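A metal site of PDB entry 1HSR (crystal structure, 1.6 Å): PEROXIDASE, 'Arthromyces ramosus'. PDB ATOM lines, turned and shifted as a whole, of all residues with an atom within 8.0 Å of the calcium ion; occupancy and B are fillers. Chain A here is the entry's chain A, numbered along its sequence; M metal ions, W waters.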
ATOM      1  N   ILE A  53     -10.612  31.680 -14.906  1.00  0.00           N
ATOM      2  CA  ILE A  53     -11.555  30.940 -15.748  1.00  0.00           C
ATOM      3  C   ILE A  53     -11.015  30.674 -17.152  1.00  0.00           C
ATOM      4  O   ILE A  53     -11.207  29.555 -17.656  1.00  0.00           O
ATOM      5  CB  ILE A  53     -12.898  31.721 -15.839  1.00  0.00           C
ATOM      6  CG1 ILE A  53     -13.636  31.569 -14.480  1.00  0.00           C
ATOM      7  CG2 ILE A  53     -13.801  31.201 -16.982  1.00  0.00           C
ATOM      8  CD1 ILE A  53     -14.814  32.593 -14.388  1.00  0.00           C
ATOM      9  N   VAL A  54     -10.325  31.607 -17.828  1.00  0.00           N
ATOM     10  CA  VAL A  54      -9.877  31.350 -19.192  1.00  0.00           C
ATOM     11  C   VAL A  54      -8.851  30.210 -19.198  1.00  0.00           C
ATOM     12  O   VAL A  54      -8.889  29.350 -20.098  1.00  0.00           O
ATOM     13  CB  VAL A  54      -9.311  32.694 -19.814  1.00  0.00           C
ATOM     14  CG1 VAL A  54      -7.933  33.126 -19.302  1.00  0.00           C
ATOM     15  CG2 VAL A  54      -9.285  32.461 -21.324  1.00  0.00           C
ATOM     16  N   PHE A  55      -7.965  30.169 -18.182  1.00  0.00           N
ATOM     17  CA  PHE A  55      -6.995  29.107 -18.042  1.00  0.00           C
ATOM     18  C   PHE A  55      -7.767  27.783 -17.811  1.00  0.00           C
ATOM     19  O   PHE A  55      -7.522  26.813 -18.532  1.00  0.00           O
ATOM     20  CB  PHE A  55      -6.052  29.403 -16.842  1.00  0.00           C
ATOM     21  CG  PHE A  55      -5.026  28.293 -16.550  1.00  0.00           C
ATOM     22  CD1 PHE A  55      -4.339  27.671 -17.605  1.00  0.00           C
ATOM     23  CD2 PHE A  55      -4.769  27.902 -15.236  1.00  0.00           C
ATOM     24  CE1 PHE A  55      -3.405  26.674 -17.337  1.00  0.00           C
ATOM     25  CE2 PHE A  55      -3.828  26.901 -14.975  1.00  0.00           C
ATOM     26  CZ  PHE A  55      -3.140  26.285 -16.017  1.00  0.00           C
ATOM     27  N   HIS A  56      -8.723  27.714 -16.879  1.00  0.00           N
ATOM     28  CA  HIS A  56      -9.429  26.464 -16.592  1.00  0.00           C
ATOM     29  C   HIS A  56     -10.341  25.976 -17.718  1.00  0.00           C
ATOM     30  O   HIS A  56     -10.615  24.765 -17.854  1.00  0.00           O
ATOM     31  CB  HIS A  56     -10.213  26.659 -15.292  1.00  0.00           C
ATOM     32  CG  HIS A  56      -9.280  26.716 -14.081  1.00  0.00           C
ATOM     33  ND1 HIS A  56      -9.735  26.705 -12.763  1.00  0.00           N
ATOM     34  CD2 HIS A  56      -7.886  26.843 -14.108  1.00  0.00           C
ATOM     35  CE1 HIS A  56      -8.638  26.880 -12.007  1.00  0.00           C
ATOM     36  NE2 HIS A  56      -7.560  26.963 -12.756  1.00  0.00           N
ATOM     37  N   ASP A  57     -10.792  26.895 -18.567  1.00  0.00           N
ATOM     38  CA  ASP A  57     -11.567  26.476 -19.717  1.00  0.00           C
ATOM     39  C   ASP A  57     -10.647  25.884 -20.781  1.00  0.00           C
ATOM     40  O   ASP A  57     -10.879  24.737 -21.216  1.00  0.00           O
ATOM     41  CB  ASP A  57     -12.330  27.645 -20.370  1.00  0.00           C
ATOM     42  CG  ASP A  57     -13.182  27.224 -21.570  1.00  0.00           C
ATOM     43  OD1 ASP A  57     -13.634  26.077 -21.602  1.00  0.00           O
ATOM     44  OD2 ASP A  57     -13.381  28.055 -22.460  1.00  0.00           O
ATOM     45  N   ALA A  58      -9.583  26.600 -21.147  1.00  0.00           N
ATOM     46  CA  ALA A  58      -8.703  26.186 -22.223  1.00  0.00           C
ATOM     47  C   ALA A  58      -7.831  24.993 -21.963  1.00  0.00           C
ATOM     48  O   ALA A  58      -7.602  24.204 -22.893  1.00  0.00           O
ATOM     49  CB  ALA A  58      -7.781  27.337 -22.631  1.00  0.00           C
ATOM     50  N   ILE A  59      -7.365  24.817 -20.721  1.00  0.00           N
ATOM     51  CA  ILE A  59      -6.459  23.724 -20.407  1.00  0.00           C
ATOM     52  C   ILE A  59      -7.141  22.358 -20.356  1.00  0.00           C
ATOM     53  O   ILE A  59      -6.450  21.347 -20.211  1.00  0.00           O
ATOM     54  CB  ILE A  59      -5.713  24.107 -19.059  1.00  0.00           C
ATOM     55  CG1 ILE A  59      -4.330  23.406 -19.024  1.00  0.00           C
ATOM     56  CG2 ILE A  59      -6.527  23.694 -17.824  1.00  0.00           C
ATOM     57  CD1 ILE A  59      -3.392  23.912 -20.121  1.00  0.00           C
ATOM     58  N   GLY A  60      -8.483  22.287 -20.500  1.00  0.00           N
ATOM     59  CA  GLY A  60      -9.193  21.022 -20.526  1.00  0.00           C
ATOM     60  C   GLY A  60      -9.061  20.524 -21.949  1.00  0.00           C
ATOM     61  O   GLY A  60     -10.022  20.514 -22.743  1.00  0.00           O
ATOM     62  N   PHE A  61      -7.833  20.126 -22.284  1.00  0.00           N
ATOM     63  CA  PHE A  61      -7.465  19.692 -23.623  1.00  0.00           C
ATOM     64  C   PHE A  61      -6.257  18.762 -23.439  1.00  0.00           C
ATOM     65  O   PHE A  61      -5.219  19.169 -22.892  1.00  0.00           O
ATOM     66  CB  PHE A  61      -7.117  20.937 -24.445  1.00  0.00           C
ATOM     67  CG  PHE A  61      -6.644  20.650 -25.843  1.00  0.00           C
ATOM     68  CD1 PHE A  61      -7.578  20.286 -26.784  1.00  0.00           C
ATOM     69  CD2 PHE A  61      -5.274  20.774 -26.164  1.00  0.00           C
ATOM     70  CE1 PHE A  61      -7.150  20.042 -28.082  1.00  0.00           C
ATOM     71  CE2 PHE A  61      -4.854  20.528 -27.469  1.00  0.00           C
ATOM     72  CZ  PHE A  61      -5.796  20.156 -28.429  1.00  0.00           C
ATOM     73  N   GLY A  73     -11.130  16.532 -24.318  1.00  0.00           N
ATOM     74  CA  GLY A  73     -11.543  17.901 -24.027  1.00  0.00           C
ATOM     75  C   GLY A  73     -11.466  18.780 -25.274  1.00  0.00           C
ATOM     76  O   GLY A  73     -10.645  18.536 -26.154  1.00  0.00           O
ATOM     77  N   GLY A  74     -12.332  19.766 -25.383  1.00  0.00           N
ATOM     78  CA  GLY A  74     -12.380  20.625 -26.544  1.00  0.00           C
ATOM     79  C   GLY A  74     -11.573  21.929 -26.408  1.00  0.00           C
ATOM     80  O   GLY A  74     -11.693  22.820 -27.267  1.00  0.00           O
ATOM     81  N   GLY A  75     -10.783  22.087 -25.332  1.00  0.00           N
ATOM     82  CA  GLY A  75      -9.957  23.267 -25.192  1.00  0.00           C
ATOM     83  C   GLY A  75     -10.750  24.526 -24.870  1.00  0.00           C
ATOM     84  O   GLY A  75     -11.617  24.478 -23.984  1.00  0.00           O
ATOM     85  N   ALA A  76     -10.537  25.619 -25.583  1.00  0.00           N
ATOM     86  CA  ALA A  76     -11.152  26.918 -25.335  1.00  0.00           C
ATOM     87  C   ALA A  76     -12.563  26.977 -25.951  1.00  0.00           C
ATOM     88  O   ALA A  76     -12.941  27.860 -26.716  1.00  0.00           O
ATOM     89  CB  ALA A  76     -10.200  28.004 -25.940  1.00  0.00           C
ATOM     90  N   ASP A  77     -13.393  26.042 -25.486  1.00  0.00           N
ATOM     91  CA  ASP A  77     -14.716  25.855 -26.030  1.00  0.00           C
ATOM     92  C   ASP A  77     -15.902  26.355 -25.190  1.00  0.00           C
ATOM     93  O   ASP A  77     -17.084  26.120 -25.538  1.00  0.00           O
ATOM     94  CB  ASP A  77     -14.856  24.343 -26.312  1.00  0.00           C
ATOM     95  CG  ASP A  77     -14.731  23.480 -25.067  1.00  0.00           C
ATOM     96  OD1 ASP A  77     -14.564  23.992 -23.970  1.00  0.00           O
ATOM     97  OD2 ASP A  77     -14.794  22.250 -25.158  1.00  0.00           O
ATOM     98  N   GLY A  78     -15.597  27.046 -24.075  1.00  0.00           N
ATOM     99  CA  GLY A  78     -16.585  27.544 -23.135  1.00  0.00           C
ATOM    100  C   GLY A  78     -17.297  26.405 -22.384  1.00  0.00           C
ATOM    101  O   GLY A  78     -18.352  26.635 -21.791  1.00  0.00           O
ATOM    102  N   SER A  79     -16.701  25.210 -22.304  1.00  0.00           N
ATOM    103  CA  SER A  79     -17.376  24.065 -21.669  1.00  0.00           C
ATOM    104  C   SER A  79     -17.532  24.332 -20.175  1.00  0.00           C
ATOM    105  O   SER A  79     -18.460  23.805 -19.561  1.00  0.00           O
ATOM    106  CB  SER A  79     -16.596  22.772 -21.857  1.00  0.00           C
ATOM    107  OG  SER A  79     -15.261  22.838 -21.304  1.00  0.00           O
ATOM    108  N   ILE A  80     -16.678  25.180 -19.576  1.00  0.00           N
ATOM    109  CA  ILE A  80     -16.801  25.479 -18.146  1.00  0.00           C
ATOM    110  C   ILE A  80     -18.093  26.199 -17.858  1.00  0.00           C
ATOM    111  O   ILE A  80     -18.565  26.147 -16.724  1.00  0.00           O
ATOM    112  CB  ILE A  80     -15.496  26.270 -17.698  1.00  0.00           C
ATOM    113  CG1 ILE A  80     -15.406  26.300 -16.160  1.00  0.00           C
ATOM    114  CG2 ILE A  80     -15.500  27.687 -18.240  1.00  0.00           C
ATOM    115  CD1 ILE A  80     -14.029  26.783 -15.633  1.00  0.00           C
ATOM    116  N   ILE A  81     -18.713  26.851 -18.848  1.00  0.00           N
ATOM    117  CA  ILE A  81     -19.997  27.519 -18.645  1.00  0.00           C
ATOM    118  C   ILE A  81     -21.103  26.555 -19.092  1.00  0.00           C
ATOM    119  O   ILE A  81     -21.999  26.237 -18.288  1.00  0.00           O
ATOM    120  CB  ILE A  81     -20.113  28.807 -19.465  1.00  0.00           C
ATOM    121  CG1 ILE A  81     -19.023  29.806 -19.043  1.00  0.00           C
ATOM    122  CG2 ILE A  81     -21.508  29.395 -19.252  1.00  0.00           C
ATOM    123  CD1 ILE A  81     -19.120  31.148 -19.748  1.00  0.00           C
ATOM    124  N   HIS A  83     -21.193  23.388 -19.411  1.00  0.00           N
ATOM    125  CA  HIS A  83     -21.190  22.209 -18.558  1.00  0.00           C
ATOM    126  C   HIS A  83     -20.671  22.552 -17.173  1.00  0.00           C
ATOM    127  O   HIS A  83     -19.997  21.736 -16.532  1.00  0.00           O
ATOM    128  CB  HIS A  83     -20.315  21.112 -19.149  1.00  0.00           C
ATOM    129  CG  HIS A  83     -20.903  20.789 -20.509  1.00  0.00           C
ATOM    130  ND1 HIS A  83     -22.153  20.219 -20.735  1.00  0.00           N
ATOM    131  CD2 HIS A  83     -20.260  21.100 -21.704  1.00  0.00           C
ATOM    132  CE1 HIS A  83     -22.253  20.185 -22.076  1.00  0.00           C
ATOM    133  NE2 HIS A  83     -21.196  20.667 -22.652  1.00  0.00           N
ATOM    134  N   GLU A  87     -18.154  20.734 -14.468  1.00  0.00           N
ATOM    135  CA  GLU A  87     -16.798  21.244 -14.266  1.00  0.00           C
ATOM    136  C   GLU A  87     -16.571  22.012 -12.965  1.00  0.00           C
ATOM    137  O   GLU A  87     -15.475  21.992 -12.407  1.00  0.00           O
ATOM    138  CB  GLU A  87     -16.362  22.145 -15.432  1.00  0.00           C
ATOM    139  CG  GLU A  87     -16.268  21.328 -16.694  1.00  0.00           C
ATOM    140  CD  GLU A  87     -15.579  21.989 -17.869  1.00  0.00           C
ATOM    141  OE1 GLU A  87     -14.763  22.887 -17.643  1.00  0.00           O
ATOM    142  OE2 GLU A  87     -15.860  21.580 -18.993  1.00  0.00           O
ATOM    143  N   GLY A 115     -17.302  30.048 -25.656  1.00  0.00           N
ATOM    144  CA  GLY A 115     -15.834  30.017 -25.807  1.00  0.00           C
ATOM    145  C   GLY A 115     -15.296  31.389 -26.237  1.00  0.00           C
ATOM    146  O   GLY A 115     -14.295  31.889 -25.692  1.00  0.00           O
ATOM    147  N   ILE A 118     -15.555  34.038 -23.247  1.00  0.00           N
ATOM    148  CA  ILE A 118     -14.513  33.989 -22.203  1.00  0.00           C
ATOM    149  C   ILE A 118     -13.234  34.648 -22.717  1.00  0.00           C
ATOM    150  O   ILE A 118     -12.607  35.417 -21.975  1.00  0.00           O
ATOM    151  CB  ILE A 118     -14.266  32.509 -21.792  1.00  0.00           C
ATOM    152  CG1 ILE A 118     -15.492  31.955 -21.017  1.00  0.00           C
ATOM    153  CG2 ILE A 118     -13.040  32.438 -20.856  1.00  0.00           C
ATOM    154  CD1 ILE A 118     -15.478  30.427 -20.776  1.00  0.00           C
ATOM    155  N   SER A 145     -20.146  22.087 -27.111  1.00  0.00           N
ATOM    156  CA  SER A 145     -19.026  21.528 -26.363  1.00  0.00           C
ATOM    157  C   SER A 145     -19.456  20.306 -25.563  1.00  0.00           C
ATOM    158  O   SER A 145     -20.639  20.011 -25.382  1.00  0.00           O
ATOM    159  CB  SER A 145     -18.452  22.564 -25.384  1.00  0.00           C
ATOM    160  OG  SER A 145     -19.433  23.003 -24.448  1.00  0.00           O
ATOM    161  N   GLN A 146     -18.465  19.542 -25.142  1.00  0.00           N
ATOM    162  CA  GLN A 146     -18.666  18.387 -24.299  1.00  0.00           C
ATOM    163  C   GLN A 146     -17.976  18.778 -22.999  1.00  0.00           C
ATOM    164  O   GLN A 146     -17.101  19.665 -22.990  1.00  0.00           O
ATOM    165  CB  GLN A 146     -17.988  17.204 -24.917  1.00  0.00           C
ATOM    166  CG  GLN A 146     -18.783  16.630 -26.071  1.00  0.00           C
ATOM    167  CD  GLN A 146     -17.877  15.936 -27.071  1.00  0.00           C
ATOM    168  OE1 GLN A 146     -17.439  16.554 -28.057  1.00  0.00           O
ATOM    169  NE2 GLN A 146     -17.537  14.656 -26.845  1.00  0.00           N
ATOM    170  N   PRO A 147     -18.301  18.172 -21.837  1.00  0.00           N
ATOM    171  CA  PRO A 147     -17.638  18.457 -20.580  1.00  0.00           C
ATOM    172  C   PRO A 147     -16.174  18.085 -20.648  1.00  0.00           C
ATOM    173  O   PRO A 147     -15.781  17.065 -21.243  1.00  0.00           O
ATOM    174  CB  PRO A 147     -18.389  17.636 -19.547  1.00  0.00           C
ATOM    175  CG  PRO A 147     -19.722  17.363 -20.205  1.00  0.00           C
ATOM    176  CD  PRO A 147     -19.355  17.187 -21.658  1.00  0.00           C
ATOM    177  N   SER A 148     -15.347  18.901 -20.009  1.00  0.00           N
ATOM    178  CA  SER A 148     -13.930  18.618 -19.929  1.00  0.00           C
ATOM    179  C   SER A 148     -13.733  17.340 -19.110  1.00  0.00           C
ATOM    180  O   SER A 148     -14.461  17.119 -18.126  1.00  0.00           O
ATOM    181  CB  SER A 148     -13.166  19.719 -19.202  1.00  0.00           C
ATOM    182  OG  SER A 148     -11.807  19.398 -18.891  1.00  0.00           O
ATOM    183  N   PRO A 149     -12.757  16.494 -19.448  1.00  0.00           N
ATOM    184  CA  PRO A 149     -12.337  15.393 -18.614  1.00  0.00           C
ATOM    185  C   PRO A 149     -11.822  15.968 -17.283  1.00  0.00           C
ATOM    186  O   PRO A 149     -11.328  17.110 -17.250  1.00  0.00           O
ATOM    187  CB  PRO A 149     -11.262  14.707 -19.408  1.00  0.00           C
ATOM    188  CG  PRO A 149     -11.714  14.969 -20.815  1.00  0.00           C
ATOM    189  CD  PRO A 149     -12.106  16.430 -20.749  1.00  0.00           C
ATOM    190  N   LEU A 283      -6.602  26.606 -28.259  1.00  0.00           N
ATOM    191  CA  LEU A 283      -6.456  25.160 -27.992  1.00  0.00           C
ATOM    192  C   LEU A 283      -7.814  24.516 -28.334  1.00  0.00           C
ATOM    193  O   LEU A 283      -8.882  25.002 -27.932  1.00  0.00           O
ATOM    194  CB  LEU A 283      -6.112  24.949 -26.509  1.00  0.00           C
ATOM    195  CG  LEU A 283      -4.692  24.636 -25.930  1.00  0.00           C
ATOM    196  CD1 LEU A 283      -3.533  25.110 -26.773  1.00  0.00           C
ATOM    197  CD2 LEU A 283      -4.677  25.214 -24.529  1.00  0.00           C
ATOM    198  N   PHE A 285      -8.872  24.436 -31.523  1.00  0.00           N
ATOM    199  CA  PHE A 285      -9.389  25.087 -32.719  1.00  0.00           C
ATOM    200  C   PHE A 285      -8.255  25.361 -33.686  1.00  0.00           C
ATOM    201  O   PHE A 285      -7.071  25.283 -33.363  1.00  0.00           O
ATOM    202  CB  PHE A 285     -10.046  26.456 -32.432  1.00  0.00           C
ATOM    203  CG  PHE A 285     -11.266  26.282 -31.539  1.00  0.00           C
ATOM    204  CD1 PHE A 285     -11.085  26.232 -30.140  1.00  0.00           C
ATOM    205  CD2 PHE A 285     -12.532  26.085 -32.112  1.00  0.00           C
ATOM    206  CE1 PHE A 285     -12.175  25.947 -29.327  1.00  0.00           C
ATOM    207  CE2 PHE A 285     -13.623  25.805 -31.286  1.00  0.00           C
ATOM    208  CZ  PHE A 285     -13.452  25.730 -29.897  1.00  0.00           C
HETATM  209 CA    CA M   1     -13.060  23.871 -21.961  1.00  0.00          CA
HETATM  210  O   HOH W   1     -12.413  21.527 -22.187  1.00  0.00           O
HETATM  211  O   HOH W   2     -12.821  23.453 -19.538  1.00  0.00           O
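The backbone NH (N) of Gly 78 lies within hydrogen-bond range of the side-chain carboxylate (OD2) of Asp 57. The side-chain carboxylate (OE2) of Glu 87 lies close to the side-chain hydroxyl (OG) of Ser 79 (2.7 Å). O of Gly 60 lies within hydrogen-bond range of N of Gly 75 (3.1 Å).
Four residues have an atom within 4 Å of the calcium ion: Asp 57, Gly 75, Asp 77 and Ser 79. The nearest printed residue that does not touch the calcium ion is Ala 58 (4.5 Å).
OD1 of Asp 57 is bound to the calcium ion (2.3 Å). The calcium ion is bound by water W1, 2.4 Å away. O of Asp 57 binds the calcium ion (2.5 Å). The calcium ion is bound by water W2 (2.5 Å). The calcium ion is bound by OD1 of Asp 77 (2.5 Å). OG of Ser 79 binds the calcium ion. O of Gly 75 binds the calcium ion (2.6 Å). The calcium ion has seven donor atoms within binding distance.
Water W2 bridges OE1 of Glu 87 (2.8 Å) and O of His 56 (3.1 Å).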
